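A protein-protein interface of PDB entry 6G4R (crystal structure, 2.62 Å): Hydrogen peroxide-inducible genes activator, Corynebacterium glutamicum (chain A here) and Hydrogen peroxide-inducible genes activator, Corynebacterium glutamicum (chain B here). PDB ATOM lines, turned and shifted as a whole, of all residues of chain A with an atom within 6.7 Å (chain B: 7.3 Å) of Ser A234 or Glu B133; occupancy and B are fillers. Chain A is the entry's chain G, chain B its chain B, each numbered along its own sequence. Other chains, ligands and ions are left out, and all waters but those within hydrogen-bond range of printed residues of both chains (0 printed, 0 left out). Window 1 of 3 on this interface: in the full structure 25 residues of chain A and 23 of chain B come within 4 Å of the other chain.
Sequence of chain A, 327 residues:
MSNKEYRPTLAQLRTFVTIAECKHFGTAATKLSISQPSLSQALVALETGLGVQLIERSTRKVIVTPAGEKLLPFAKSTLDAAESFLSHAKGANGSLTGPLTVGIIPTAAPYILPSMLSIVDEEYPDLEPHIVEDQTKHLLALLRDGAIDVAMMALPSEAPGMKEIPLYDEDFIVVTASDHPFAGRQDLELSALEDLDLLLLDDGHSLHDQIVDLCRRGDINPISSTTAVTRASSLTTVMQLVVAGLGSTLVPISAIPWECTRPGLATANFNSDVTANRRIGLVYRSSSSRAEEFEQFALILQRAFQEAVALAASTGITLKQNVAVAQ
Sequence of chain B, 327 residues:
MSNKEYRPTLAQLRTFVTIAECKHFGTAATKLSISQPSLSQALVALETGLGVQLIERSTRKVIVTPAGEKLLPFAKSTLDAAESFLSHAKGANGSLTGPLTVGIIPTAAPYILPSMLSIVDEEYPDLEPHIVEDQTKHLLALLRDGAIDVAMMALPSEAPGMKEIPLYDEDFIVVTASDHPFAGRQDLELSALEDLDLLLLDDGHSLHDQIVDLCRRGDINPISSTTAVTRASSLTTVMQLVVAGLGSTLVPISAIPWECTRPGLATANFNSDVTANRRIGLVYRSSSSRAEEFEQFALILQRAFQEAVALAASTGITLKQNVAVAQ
The backbone NH (N) of Arg A231 lies within hydrogen-bond range of the backbone carbonyl oxygen (O) of Ile B131 (3.0 Å).
The backbone NH (N) of Glu B133 lies within hydrogen-bond range of the backbone carbonyl oxygen (O) of Arg A231, 3.1 Å away.
The side-chain carboxylate (OE1) of Glu B133 lies within hydrogen-bond range of the backbone NH (N) of Ser A233 (2.7 Å).
OE1 of Glu B133 is in hydrogen-bond range of N of Ser A234.
The side-chain carboxylate (OE2) of Glu B133 lies within hydrogen-bond range of the side-chain hydroxyl (OG1) of Thr A237.
The side-chain carboxylate (OD2) of Asp B134 is in salt-bridge range of the guanidinium group (NH1) of Arg A231 (3.4 Å).
The backbone carbonyl oxygen (O) of Val B102 is in hydrogen-bond range of the backbone NH (N) of Val B132, 3.0 Å away.
The backbone NH (N) of Ile B104 sits at hydrogen-bond distance from the backbone carbonyl oxygen (O) of Val B132, at 3.0 Å.
The backbone NH (N) of Asp B134 lies within hydrogen-bond range of the backbone carbonyl oxygen (O) of Ile B104, at 3.5 Å.
OG1 of Thr A237 is in hydrogen-bond range of OG of Ser A234.
Val B132 touches Arg A231 (CA to O, 3.5 Å).
Ala A232 touches Glu B133.
Thr A236 touches Pro B110 (OG1 to CB, 3.9 Å).
Thr A237 touches Pro B110.
CD1 of Leu B113 touches CG2 of Thr A237 (3.9 Å).
Ser A234 touches just one residue of chain B: Glu B133.
Glu B133 touches just these residues of chain A: Arg A231, Ala A232, Ser A233, Ser A234 and Thr A237.
Printed residues of chain A within 4 Å of Asp B134: Arg A231 (3.4 Å).
Of the printed residues of chain B, Thr A237 touches Pro B110, Leu B113 and Glu B133.
Printed residues of chain A within 4 Å of Pro B110: Thr A236 (3.9 Å) and Thr A237 (3.5 Å).
The nearest residue of chain A that does not touch Glu B133 is Val A238 (5.7 Å).
Hydrophobic or aromatic side chains of chain B within 4 Å of the printed part of chain A: Pro B110, Leu B113 and Val B132.
Along chain B the printed residues that touch a printed residue of chain A span positions 110 to 134.
Of the 10 printed residues of chain A, 6 touch a printed residue of chain B.
Hydrophobic or aromatic side chains of chain A within 4 Å of the printed part of chain B: Ala A232.
Among the printed residues, 11 pairs touch across the chains.
Among the printed residues, Asp or Glu carboxylates within 4 Å of a Lys or Arg side-chain nitrogen of the other chain: Arg A231 with Asp B134 (3.4 Å).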
ATOM      1  N   LEU A 201     -21.690   3.608 -22.492  1.00  0.00           N
ATOM      2  CA  LEU A 201     -22.821   3.858 -21.612  1.00  0.00           C
ATOM      3  C   LEU A 201     -23.788   2.691 -21.764  1.00  0.00           C
ATOM      4  O   LEU A 201     -24.040   2.225 -22.879  1.00  0.00           O
ATOM      5  CB  LEU A 201     -23.512   5.188 -21.933  1.00  0.00           C
ATOM      6  CG  LEU A 201     -22.860   6.529 -21.559  1.00  0.00           C
ATOM      7  CD1 LEU A 201     -22.907   6.722 -20.047  1.00  0.00           C
ATOM      8  CD2 LEU A 201     -21.432   6.687 -22.070  1.00  0.00           C
ATOM      9  N   ARG A 231     -13.241   4.819 -17.866  1.00  0.00           N
ATOM     10  CA  ARG A 231     -14.685   4.908 -17.692  1.00  0.00           C
ATOM     11  C   ARG A 231     -15.104   6.364 -17.821  1.00  0.00           C
ATOM     12  O   ARG A 231     -14.570   7.226 -17.118  1.00  0.00           O
ATOM     13  CB  ARG A 231     -15.116   4.359 -16.329  1.00  0.00           C
ATOM     14  CG  ARG A 231     -16.616   4.183 -16.181  1.00  0.00           C
ATOM     15  CD  ARG A 231     -16.957   3.478 -14.881  1.00  0.00           C
ATOM     16  NE  ARG A 231     -16.233   4.059 -13.754  1.00  0.00           N
ATOM     17  CZ  ARG A 231     -16.615   5.155 -13.104  1.00  0.00           C
ATOM     18  NH1 ARG A 231     -17.718   5.794 -13.469  1.00  0.00           N
ATOM     19  NH2 ARG A 231     -15.893   5.614 -12.090  1.00  0.00           N
ATOM     20  N   ALA A 232     -16.056   6.632 -18.711  1.00  0.00           N
ATOM     21  CA  ALA A 232     -16.571   7.973 -18.927  1.00  0.00           C
ATOM     22  C   ALA A 232     -18.058   8.017 -18.596  1.00  0.00           C
ATOM     23  O   ALA A 232     -18.745   6.992 -18.578  1.00  0.00           O
ATOM     24  CB  ALA A 232     -16.339   8.435 -20.371  1.00  0.00           C
ATOM     25  N   SER A 233     -18.551   9.229 -18.333  1.00  0.00           N
ATOM     26  CA  SER A 233     -19.944   9.436 -17.965  1.00  0.00           C
ATOM     27  C   SER A 233     -20.771  10.111 -19.051  1.00  0.00           C
ATOM     28  O   SER A 233     -21.995  10.192 -18.908  1.00  0.00           O
ATOM     29  CB  SER A 233     -20.033  10.268 -16.677  1.00  0.00           C
ATOM     30  OG  SER A 233     -19.674  11.618 -16.916  1.00  0.00           O
ATOM     31  N   SER A 234     -20.147  10.591 -20.125  1.00  0.00           N
ATOM     32  CA  SER A 234     -20.860  11.287 -21.184  1.00  0.00           C
ATOM     33  C   SER A 234     -20.354  10.806 -22.537  1.00  0.00           C
ATOM     34  O   SER A 234     -19.213  10.356 -22.668  1.00  0.00           O
ATOM     35  CB  SER A 234     -20.695  12.808 -21.070  1.00  0.00           C
ATOM     36  OG  SER A 234     -19.359  13.196 -21.333  1.00  0.00           O
ATOM     37  N   LEU A 235     -21.225  10.906 -23.545  1.00  0.00           N
ATOM     38  CA  LEU A 235     -20.849  10.487 -24.892  1.00  0.00           C
ATOM     39  C   LEU A 235     -19.749  11.371 -25.464  1.00  0.00           C
ATOM     40  O   LEU A 235     -18.858  10.882 -26.167  1.00  0.00           O
ATOM     41  CB  LEU A 235     -22.074  10.494 -25.807  1.00  0.00           C
ATOM     42  CG  LEU A 235     -22.908   9.212 -25.811  1.00  0.00           C
ATOM     43  CD1 LEU A 235     -24.131   9.363 -26.702  1.00  0.00           C
ATOM     44  CD2 LEU A 235     -22.062   8.029 -26.253  1.00  0.00           C
ATOM     45  N   THR A 236     -19.798  12.677 -25.184  1.00  0.00           N
ATOM     46  CA  THR A 236     -18.786  13.580 -25.720  1.00  0.00           C
ATOM     47  C   THR A 236     -17.397  13.250 -25.184  1.00  0.00           C
ATOM     48  O   THR A 236     -16.399  13.453 -25.885  1.00  0.00           O
ATOM     49  CB  THR A 236     -19.153  15.036 -25.412  1.00  0.00           C
ATOM     50  OG1 THR A 236     -18.159  15.910 -25.962  1.00  0.00           O
ATOM     51  CG2 THR A 236     -19.261  15.268 -23.910  1.00  0.00           C
ATOM     52  N   THR A 237     -17.310  12.738 -23.955  1.00  0.00           N
ATOM     53  CA  THR A 237     -16.024  12.301 -23.424  1.00  0.00           C
ATOM     54  C   THR A 237     -15.599  10.974 -24.041  1.00  0.00           C
ATOM     55  O   THR A 237     -14.417  10.779 -24.349  1.00  0.00           O
ATOM     56  CB  THR A 237     -16.090  12.187 -21.900  1.00  0.00           C
ATOM     57  OG1 THR A 237     -16.446  13.457 -21.341  1.00  0.00           O
ATOM     58  CG2 THR A 237     -14.744  11.757 -21.336  1.00  0.00           C
ATOM     59  N   VAL A 238     -16.550  10.054 -24.227  1.00  0.00           N
ATOM     60  CA  VAL A 238     -16.248   8.786 -24.885  1.00  0.00           C
ATOM     61  C   VAL A 238     -15.706   9.032 -26.286  1.00  0.00           C
ATOM     62  O   VAL A 238     -14.775   8.351 -26.736  1.00  0.00           O
ATOM     63  CB  VAL A 238     -17.498   7.886 -24.913  1.00  0.00           C
ATOM     64  CG1 VAL A 238     -17.258   6.660 -25.782  1.00  0.00           C
ATOM     65  CG2 VAL A 238     -17.885   7.470 -23.505  1.00  0.00           C
ATOM     66  N   MET A 239     -16.269  10.016 -26.992  1.00  0.00           N
ATOM     67  CA  MET A 239     -15.812  10.303 -28.347  1.00  0.00           C
ATOM     68  C   MET A 239     -14.349  10.721 -28.362  1.00  0.00           C
ATOM     69  O   MET A 239     -13.576  10.244 -29.199  1.00  0.00           O
ATOM     70  CB  MET A 239     -16.683  11.387 -28.982  1.00  0.00           C
ATOM     71  CG  MET A 239     -18.056  10.902 -29.394  1.00  0.00           C
ATOM     72  SD  MET A 239     -17.958   9.326 -30.262  1.00  0.00           S
ATOM     73  CE  MET A 239     -19.625   9.184 -30.889  1.00  0.00           C
ATOM     74  N   VAL B 102      -6.166   8.878 -13.548  1.00  0.00           N
ATOM     75  CA  VAL B 102      -6.491  10.276 -13.290  1.00  0.00           C
ATOM     76  C   VAL B 102      -8.002  10.445 -13.322  1.00  0.00           C
ATOM     77  O   VAL B 102      -8.685   9.857 -14.171  1.00  0.00           O
ATOM     78  CB  VAL B 102      -5.809  11.200 -14.317  1.00  0.00           C
ATOM     79  CG1 VAL B 102      -6.081  12.662 -13.994  1.00  0.00           C
ATOM     80  CG2 VAL B 102      -4.313  10.927 -14.366  1.00  0.00           C
ATOM     81  N   GLY B 103      -8.526  11.238 -12.392  1.00  0.00           N
ATOM     82  CA  GLY B 103      -9.939  11.562 -12.341  1.00  0.00           C
ATOM     83  C   GLY B 103     -10.151  13.007 -12.762  1.00  0.00           C
ATOM     84  O   GLY B 103      -9.432  13.903 -12.318  1.00  0.00           O
ATOM     85  N   ILE B 104     -11.136  13.214 -13.632  1.00  0.00           N
ATOM     86  CA  ILE B 104     -11.437  14.533 -14.175  1.00  0.00           C
ATOM     87  C   ILE B 104     -12.929  14.792 -14.040  1.00  0.00           C
ATOM     88  O   ILE B 104     -13.749  13.900 -14.282  1.00  0.00           O
ATOM     89  CB  ILE B 104     -10.999  14.658 -15.650  1.00  0.00           C
ATOM     90  CG1 ILE B 104      -9.572  14.138 -15.838  1.00  0.00           C
ATOM     91  CG2 ILE B 104     -11.073  16.106 -16.101  1.00  0.00           C
ATOM     92  CD1 ILE B 104      -9.107  14.133 -17.277  1.00  0.00           C
ATOM     93  N   ILE B 105     -13.278  16.015 -13.651  1.00  0.00           N
ATOM     94  CA  ILE B 105     -14.674  16.438 -13.542  1.00  0.00           C
ATOM     95  C   ILE B 105     -15.282  16.483 -14.941  1.00  0.00           C
ATOM     96  O   ILE B 105     -14.557  16.719 -15.920  1.00  0.00           O
ATOM     97  CB  ILE B 105     -14.789  17.793 -12.826  1.00  0.00           C
ATOM     98  CG1 ILE B 105     -13.909  18.840 -13.511  1.00  0.00           C
ATOM     99  CG2 ILE B 105     -14.415  17.652 -11.357  1.00  0.00           C
ATOM    100  CD1 ILE B 105     -13.978  20.208 -12.867  1.00  0.00           C
ATOM    101  N   PRO B 106     -16.594  16.272 -15.088  1.00  0.00           N
ATOM    102  CA  PRO B 106     -17.171  16.172 -16.439  1.00  0.00           C
ATOM    103  C   PRO B 106     -17.175  17.478 -17.216  1.00  0.00           C
ATOM    104  O   PRO B 106     -17.215  17.436 -18.452  1.00  0.00           O
ATOM    105  CB  PRO B 106     -18.604  15.678 -16.182  1.00  0.00           C
ATOM    106  CG  PRO B 106     -18.623  15.207 -14.760  1.00  0.00           C
ATOM    107  CD  PRO B 106     -17.588  16.000 -14.038  1.00  0.00           C
ATOM    108  N   THR B 107     -17.135  18.630 -16.550  1.00  0.00           N
ATOM    109  CA  THR B 107     -17.111  19.903 -17.260  1.00  0.00           C
ATOM    110  C   THR B 107     -15.721  20.276 -17.759  1.00  0.00           C
ATOM    111  O   THR B 107     -15.551  21.364 -18.318  1.00  0.00           O
ATOM    112  CB  THR B 107     -17.651  21.024 -16.368  1.00  0.00           C
ATOM    113  OG1 THR B 107     -16.876  21.098 -15.165  1.00  0.00           O
ATOM    114  CG2 THR B 107     -19.110  20.768 -16.019  1.00  0.00           C
ATOM    115  N   ALA B 108     -14.732  19.406 -17.569  1.00  0.00           N
ATOM    116  CA  ALA B 108     -13.384  19.638 -18.069  1.00  0.00           C
ATOM    117  C   ALA B 108     -12.806  18.465 -18.845  1.00  0.00           C
ATOM    118  O   ALA B 108     -11.878  18.678 -19.633  1.00  0.00           O
ATOM    119  CB  ALA B 108     -12.432  19.982 -16.914  1.00  0.00           C
ATOM    120  N   ALA B 109     -13.313  17.242 -18.648  1.00  0.00           N
ATOM    121  CA  ALA B 109     -12.726  16.068 -19.293  1.00  0.00           C
ATOM    122  C   ALA B 109     -12.741  16.153 -20.815  1.00  0.00           C
ATOM    123  O   ALA B 109     -11.661  16.102 -21.427  1.00  0.00           O
ATOM    124  CB  ALA B 109     -13.421  14.805 -18.776  1.00  0.00           C
ATOM    125  N   PRO B 110     -13.892  16.285 -21.490  1.00  0.00           N
ATOM    126  CA  PRO B 110     -13.879  16.199 -22.960  1.00  0.00           C
ATOM    127  C   PRO B 110     -13.182  17.367 -23.635  1.00  0.00           C
ATOM    128  O   PRO B 110     -12.934  17.299 -24.847  1.00  0.00           O
ATOM    129  CB  PRO B 110     -15.368  16.164 -23.319  1.00  0.00           C
ATOM    130  CG  PRO B 110     -16.012  16.952 -22.245  1.00  0.00           C
ATOM    131  CD  PRO B 110     -15.228  16.666 -20.989  1.00  0.00           C
ATOM    132  N   LEU B 113      -8.959  16.416 -22.596  1.00  0.00           N
ATOM    133  CA  LEU B 113      -8.395  15.123 -22.982  1.00  0.00           C
ATOM    134  C   LEU B 113      -7.694  15.131 -24.336  1.00  0.00           C
ATOM    135  O   LEU B 113      -6.597  14.553 -24.432  1.00  0.00           O
ATOM    136  CB  LEU B 113      -9.490  14.051 -22.939  1.00  0.00           C
ATOM    137  CG  LEU B 113      -9.829  13.487 -21.559  1.00  0.00           C
ATOM    138  CD1 LEU B 113     -10.914  12.426 -21.662  1.00  0.00           C
ATOM    139  CD2 LEU B 113      -8.584  12.923 -20.894  1.00  0.00           C
ATOM    140  N   ILE B 131      -8.444   7.101 -17.589  1.00  0.00           N
ATOM    141  CA  ILE B 131      -9.309   8.257 -17.385  1.00  0.00           C
ATOM    142  C   ILE B 131     -10.560   7.815 -16.641  1.00  0.00           C
ATOM    143  O   ILE B 131     -11.177   6.800 -16.992  1.00  0.00           O
ATOM    144  CB  ILE B 131      -9.674   8.920 -18.723  1.00  0.00           C
ATOM    145  CG1 ILE B 131      -8.425   9.097 -19.587  1.00  0.00           C
ATOM    146  CG2 ILE B 131     -10.353  10.259 -18.483  1.00  0.00           C
ATOM    147  CD1 ILE B 131      -7.375   9.994 -18.973  1.00  0.00           C
ATOM    148  N   VAL B 132     -10.934   8.574 -15.615  1.00  0.00           N
ATOM    149  CA  VAL B 132     -12.157   8.342 -14.852  1.00  0.00           C
ATOM    150  C   VAL B 132     -12.907   9.666 -14.783  1.00  0.00           C
ATOM    151  O   VAL B 132     -12.440  10.614 -14.139  1.00  0.00           O
ATOM    152  CB  VAL B 132     -11.875   7.801 -13.443  1.00  0.00           C
ATOM    153  CG1 VAL B 132     -13.158   7.758 -12.626  1.00  0.00           C
ATOM    154  CG2 VAL B 132     -11.245   6.420 -13.523  1.00  0.00           C
ATOM    155  N   GLU B 133     -14.060   9.734 -15.442  1.00  0.00           N
ATOM    156  CA  GLU B 133     -14.884  10.936 -15.463  1.00  0.00           C
ATOM    157  C   GLU B 133     -16.078  10.740 -14.536  1.00  0.00           C
ATOM    158  O   GLU B 133     -16.924   9.873 -14.784  1.00  0.00           O
ATOM    159  CB  GLU B 133     -15.356  11.258 -16.880  1.00  0.00           C
ATOM    160  CG  GLU B 133     -16.189  12.528 -16.970  1.00  0.00           C
ATOM    161  CD  GLU B 133     -16.969  12.630 -18.265  1.00  0.00           C
ATOM    162  OE1 GLU B 133     -17.407  11.580 -18.781  1.00  0.00           O
ATOM    163  OE2 GLU B 133     -17.147  13.760 -18.767  1.00  0.00           O
ATOM    164  N   ASP B 134     -16.144  11.543 -13.479  1.00  0.00           N
ATOM    165  CA  ASP B 134     -17.274  11.514 -12.559  1.00  0.00           C
ATOM    166  C   ASP B 134     -17.305  12.834 -11.798  1.00  0.00           C
ATOM    167  O   ASP B 134     -16.413  13.676 -11.936  1.00  0.00           O
ATOM    168  CB  ASP B 134     -17.190  10.314 -11.612  1.00  0.00           C
ATOM    169  CG  ASP B 134     -18.542   9.673 -11.365  1.00  0.00           C
ATOM    170  OD1 ASP B 134     -19.495  10.411 -11.036  1.00  0.00           O
ATOM    171  OD2 ASP B 134     -18.654   8.435 -11.500  1.00  0.00           O
ATOM    172  N   GLN B 135     -18.346  13.007 -10.988  1.00  0.00           N
ATOM    173  CA  GLN B 135     -18.534  14.247 -10.253  1.00  0.00           C
ATOM    174  C   GLN B 135     -17.479  14.386  -9.154  1.00  0.00           C
ATOM    175  O   GLN B 135     -16.740  13.450  -8.835  1.00  0.00           O
ATOM    176  CB  GLN B 135     -19.943  14.308  -9.666  1.00  0.00           C
ATOM    177  CG  GLN B 135     -21.037  14.159 -10.711  1.00  0.00           C
ATOM    178  CD  GLN B 135     -22.423  14.109 -10.107  1.00  0.00           C
ATOM    179  OE1 GLN B 135     -22.663  14.641  -9.024  1.00  0.00           O
ATOM    180  NE2 GLN B 135     -23.349  13.462 -10.808  1.00  0.00           N
ATOM    181  N   LEU B 139     -15.163  11.533  -7.103  1.00  0.00           N
ATOM    182  CA  LEU B 139     -13.720  11.526  -7.323  1.00  0.00           C
ATOM    183  C   LEU B 139     -12.959  11.514  -6.003  1.00  0.00           C
ATOM    184  O   LEU B 139     -12.022  10.728  -5.822  1.00  0.00           O
ATOM    185  CB  LEU B 139     -13.308  12.735  -8.167  1.00  0.00           C
ATOM    186  CG  LEU B 139     -13.687  12.710  -9.648  1.00  0.00           C
ATOM    187  CD1 LEU B 139     -13.030  13.869 -10.382  1.00  0.00           C
ATOM    188  CD2 LEU B 139     -13.304  11.383 -10.282  1.00  0.00           C
ATOM    189  N   SER B 233     -28.063  17.490 -16.969  1.00  0.00           N
ATOM    190  CA  SER B 233     -26.856  16.886 -16.424  1.00  0.00           C
ATOM    191  C   SER B 233     -25.626  17.086 -17.297  1.00  0.00           C
ATOM    192  O   SER B 233     -24.518  16.757 -16.857  1.00  0.00           O
ATOM    193  CB  SER B 233     -27.070  15.383 -16.195  1.00  0.00           C
ATOM    194  OG  SER B 233     -27.119  14.680 -17.423  1.00  0.00           O
ATOM    195  N   SER B 234     -25.778  17.616 -18.509  1.00  0.00           N
ATOM    196  CA  SER B 234     -24.657  17.798 -19.418  1.00  0.00           C
ATOM    197  C   SER B 234     -24.749  19.164 -20.081  1.00  0.00           C
ATOM    198  O   SER B 234     -25.835  19.731 -20.227  1.00  0.00           O
ATOM    199  CB  SER B 234     -24.615  16.698 -20.489  1.00  0.00           C
ATOM    200  OG  SER B 234     -25.711  16.810 -21.379  1.00  0.00           O
ATOM    201  N   THR B 236     -24.096  19.844 -23.232  1.00  0.00           N
ATOM    202  CA  THR B 236     -24.709  19.752 -24.554  1.00  0.00           C
ATOM    203  C   THR B 236     -26.231  19.808 -24.477  1.00  0.00           C
ATOM    204  O   THR B 236     -26.878  20.305 -25.405  1.00  0.00           O
ATOM    205  CB  THR B 236     -24.250  18.475 -25.264  1.00  0.00           C
ATOM    206  OG1 THR B 236     -24.847  18.407 -26.565  1.00  0.00           O
ATOM    207  CG2 THR B 236     -24.634  17.237 -24.464  1.00  0.00           C
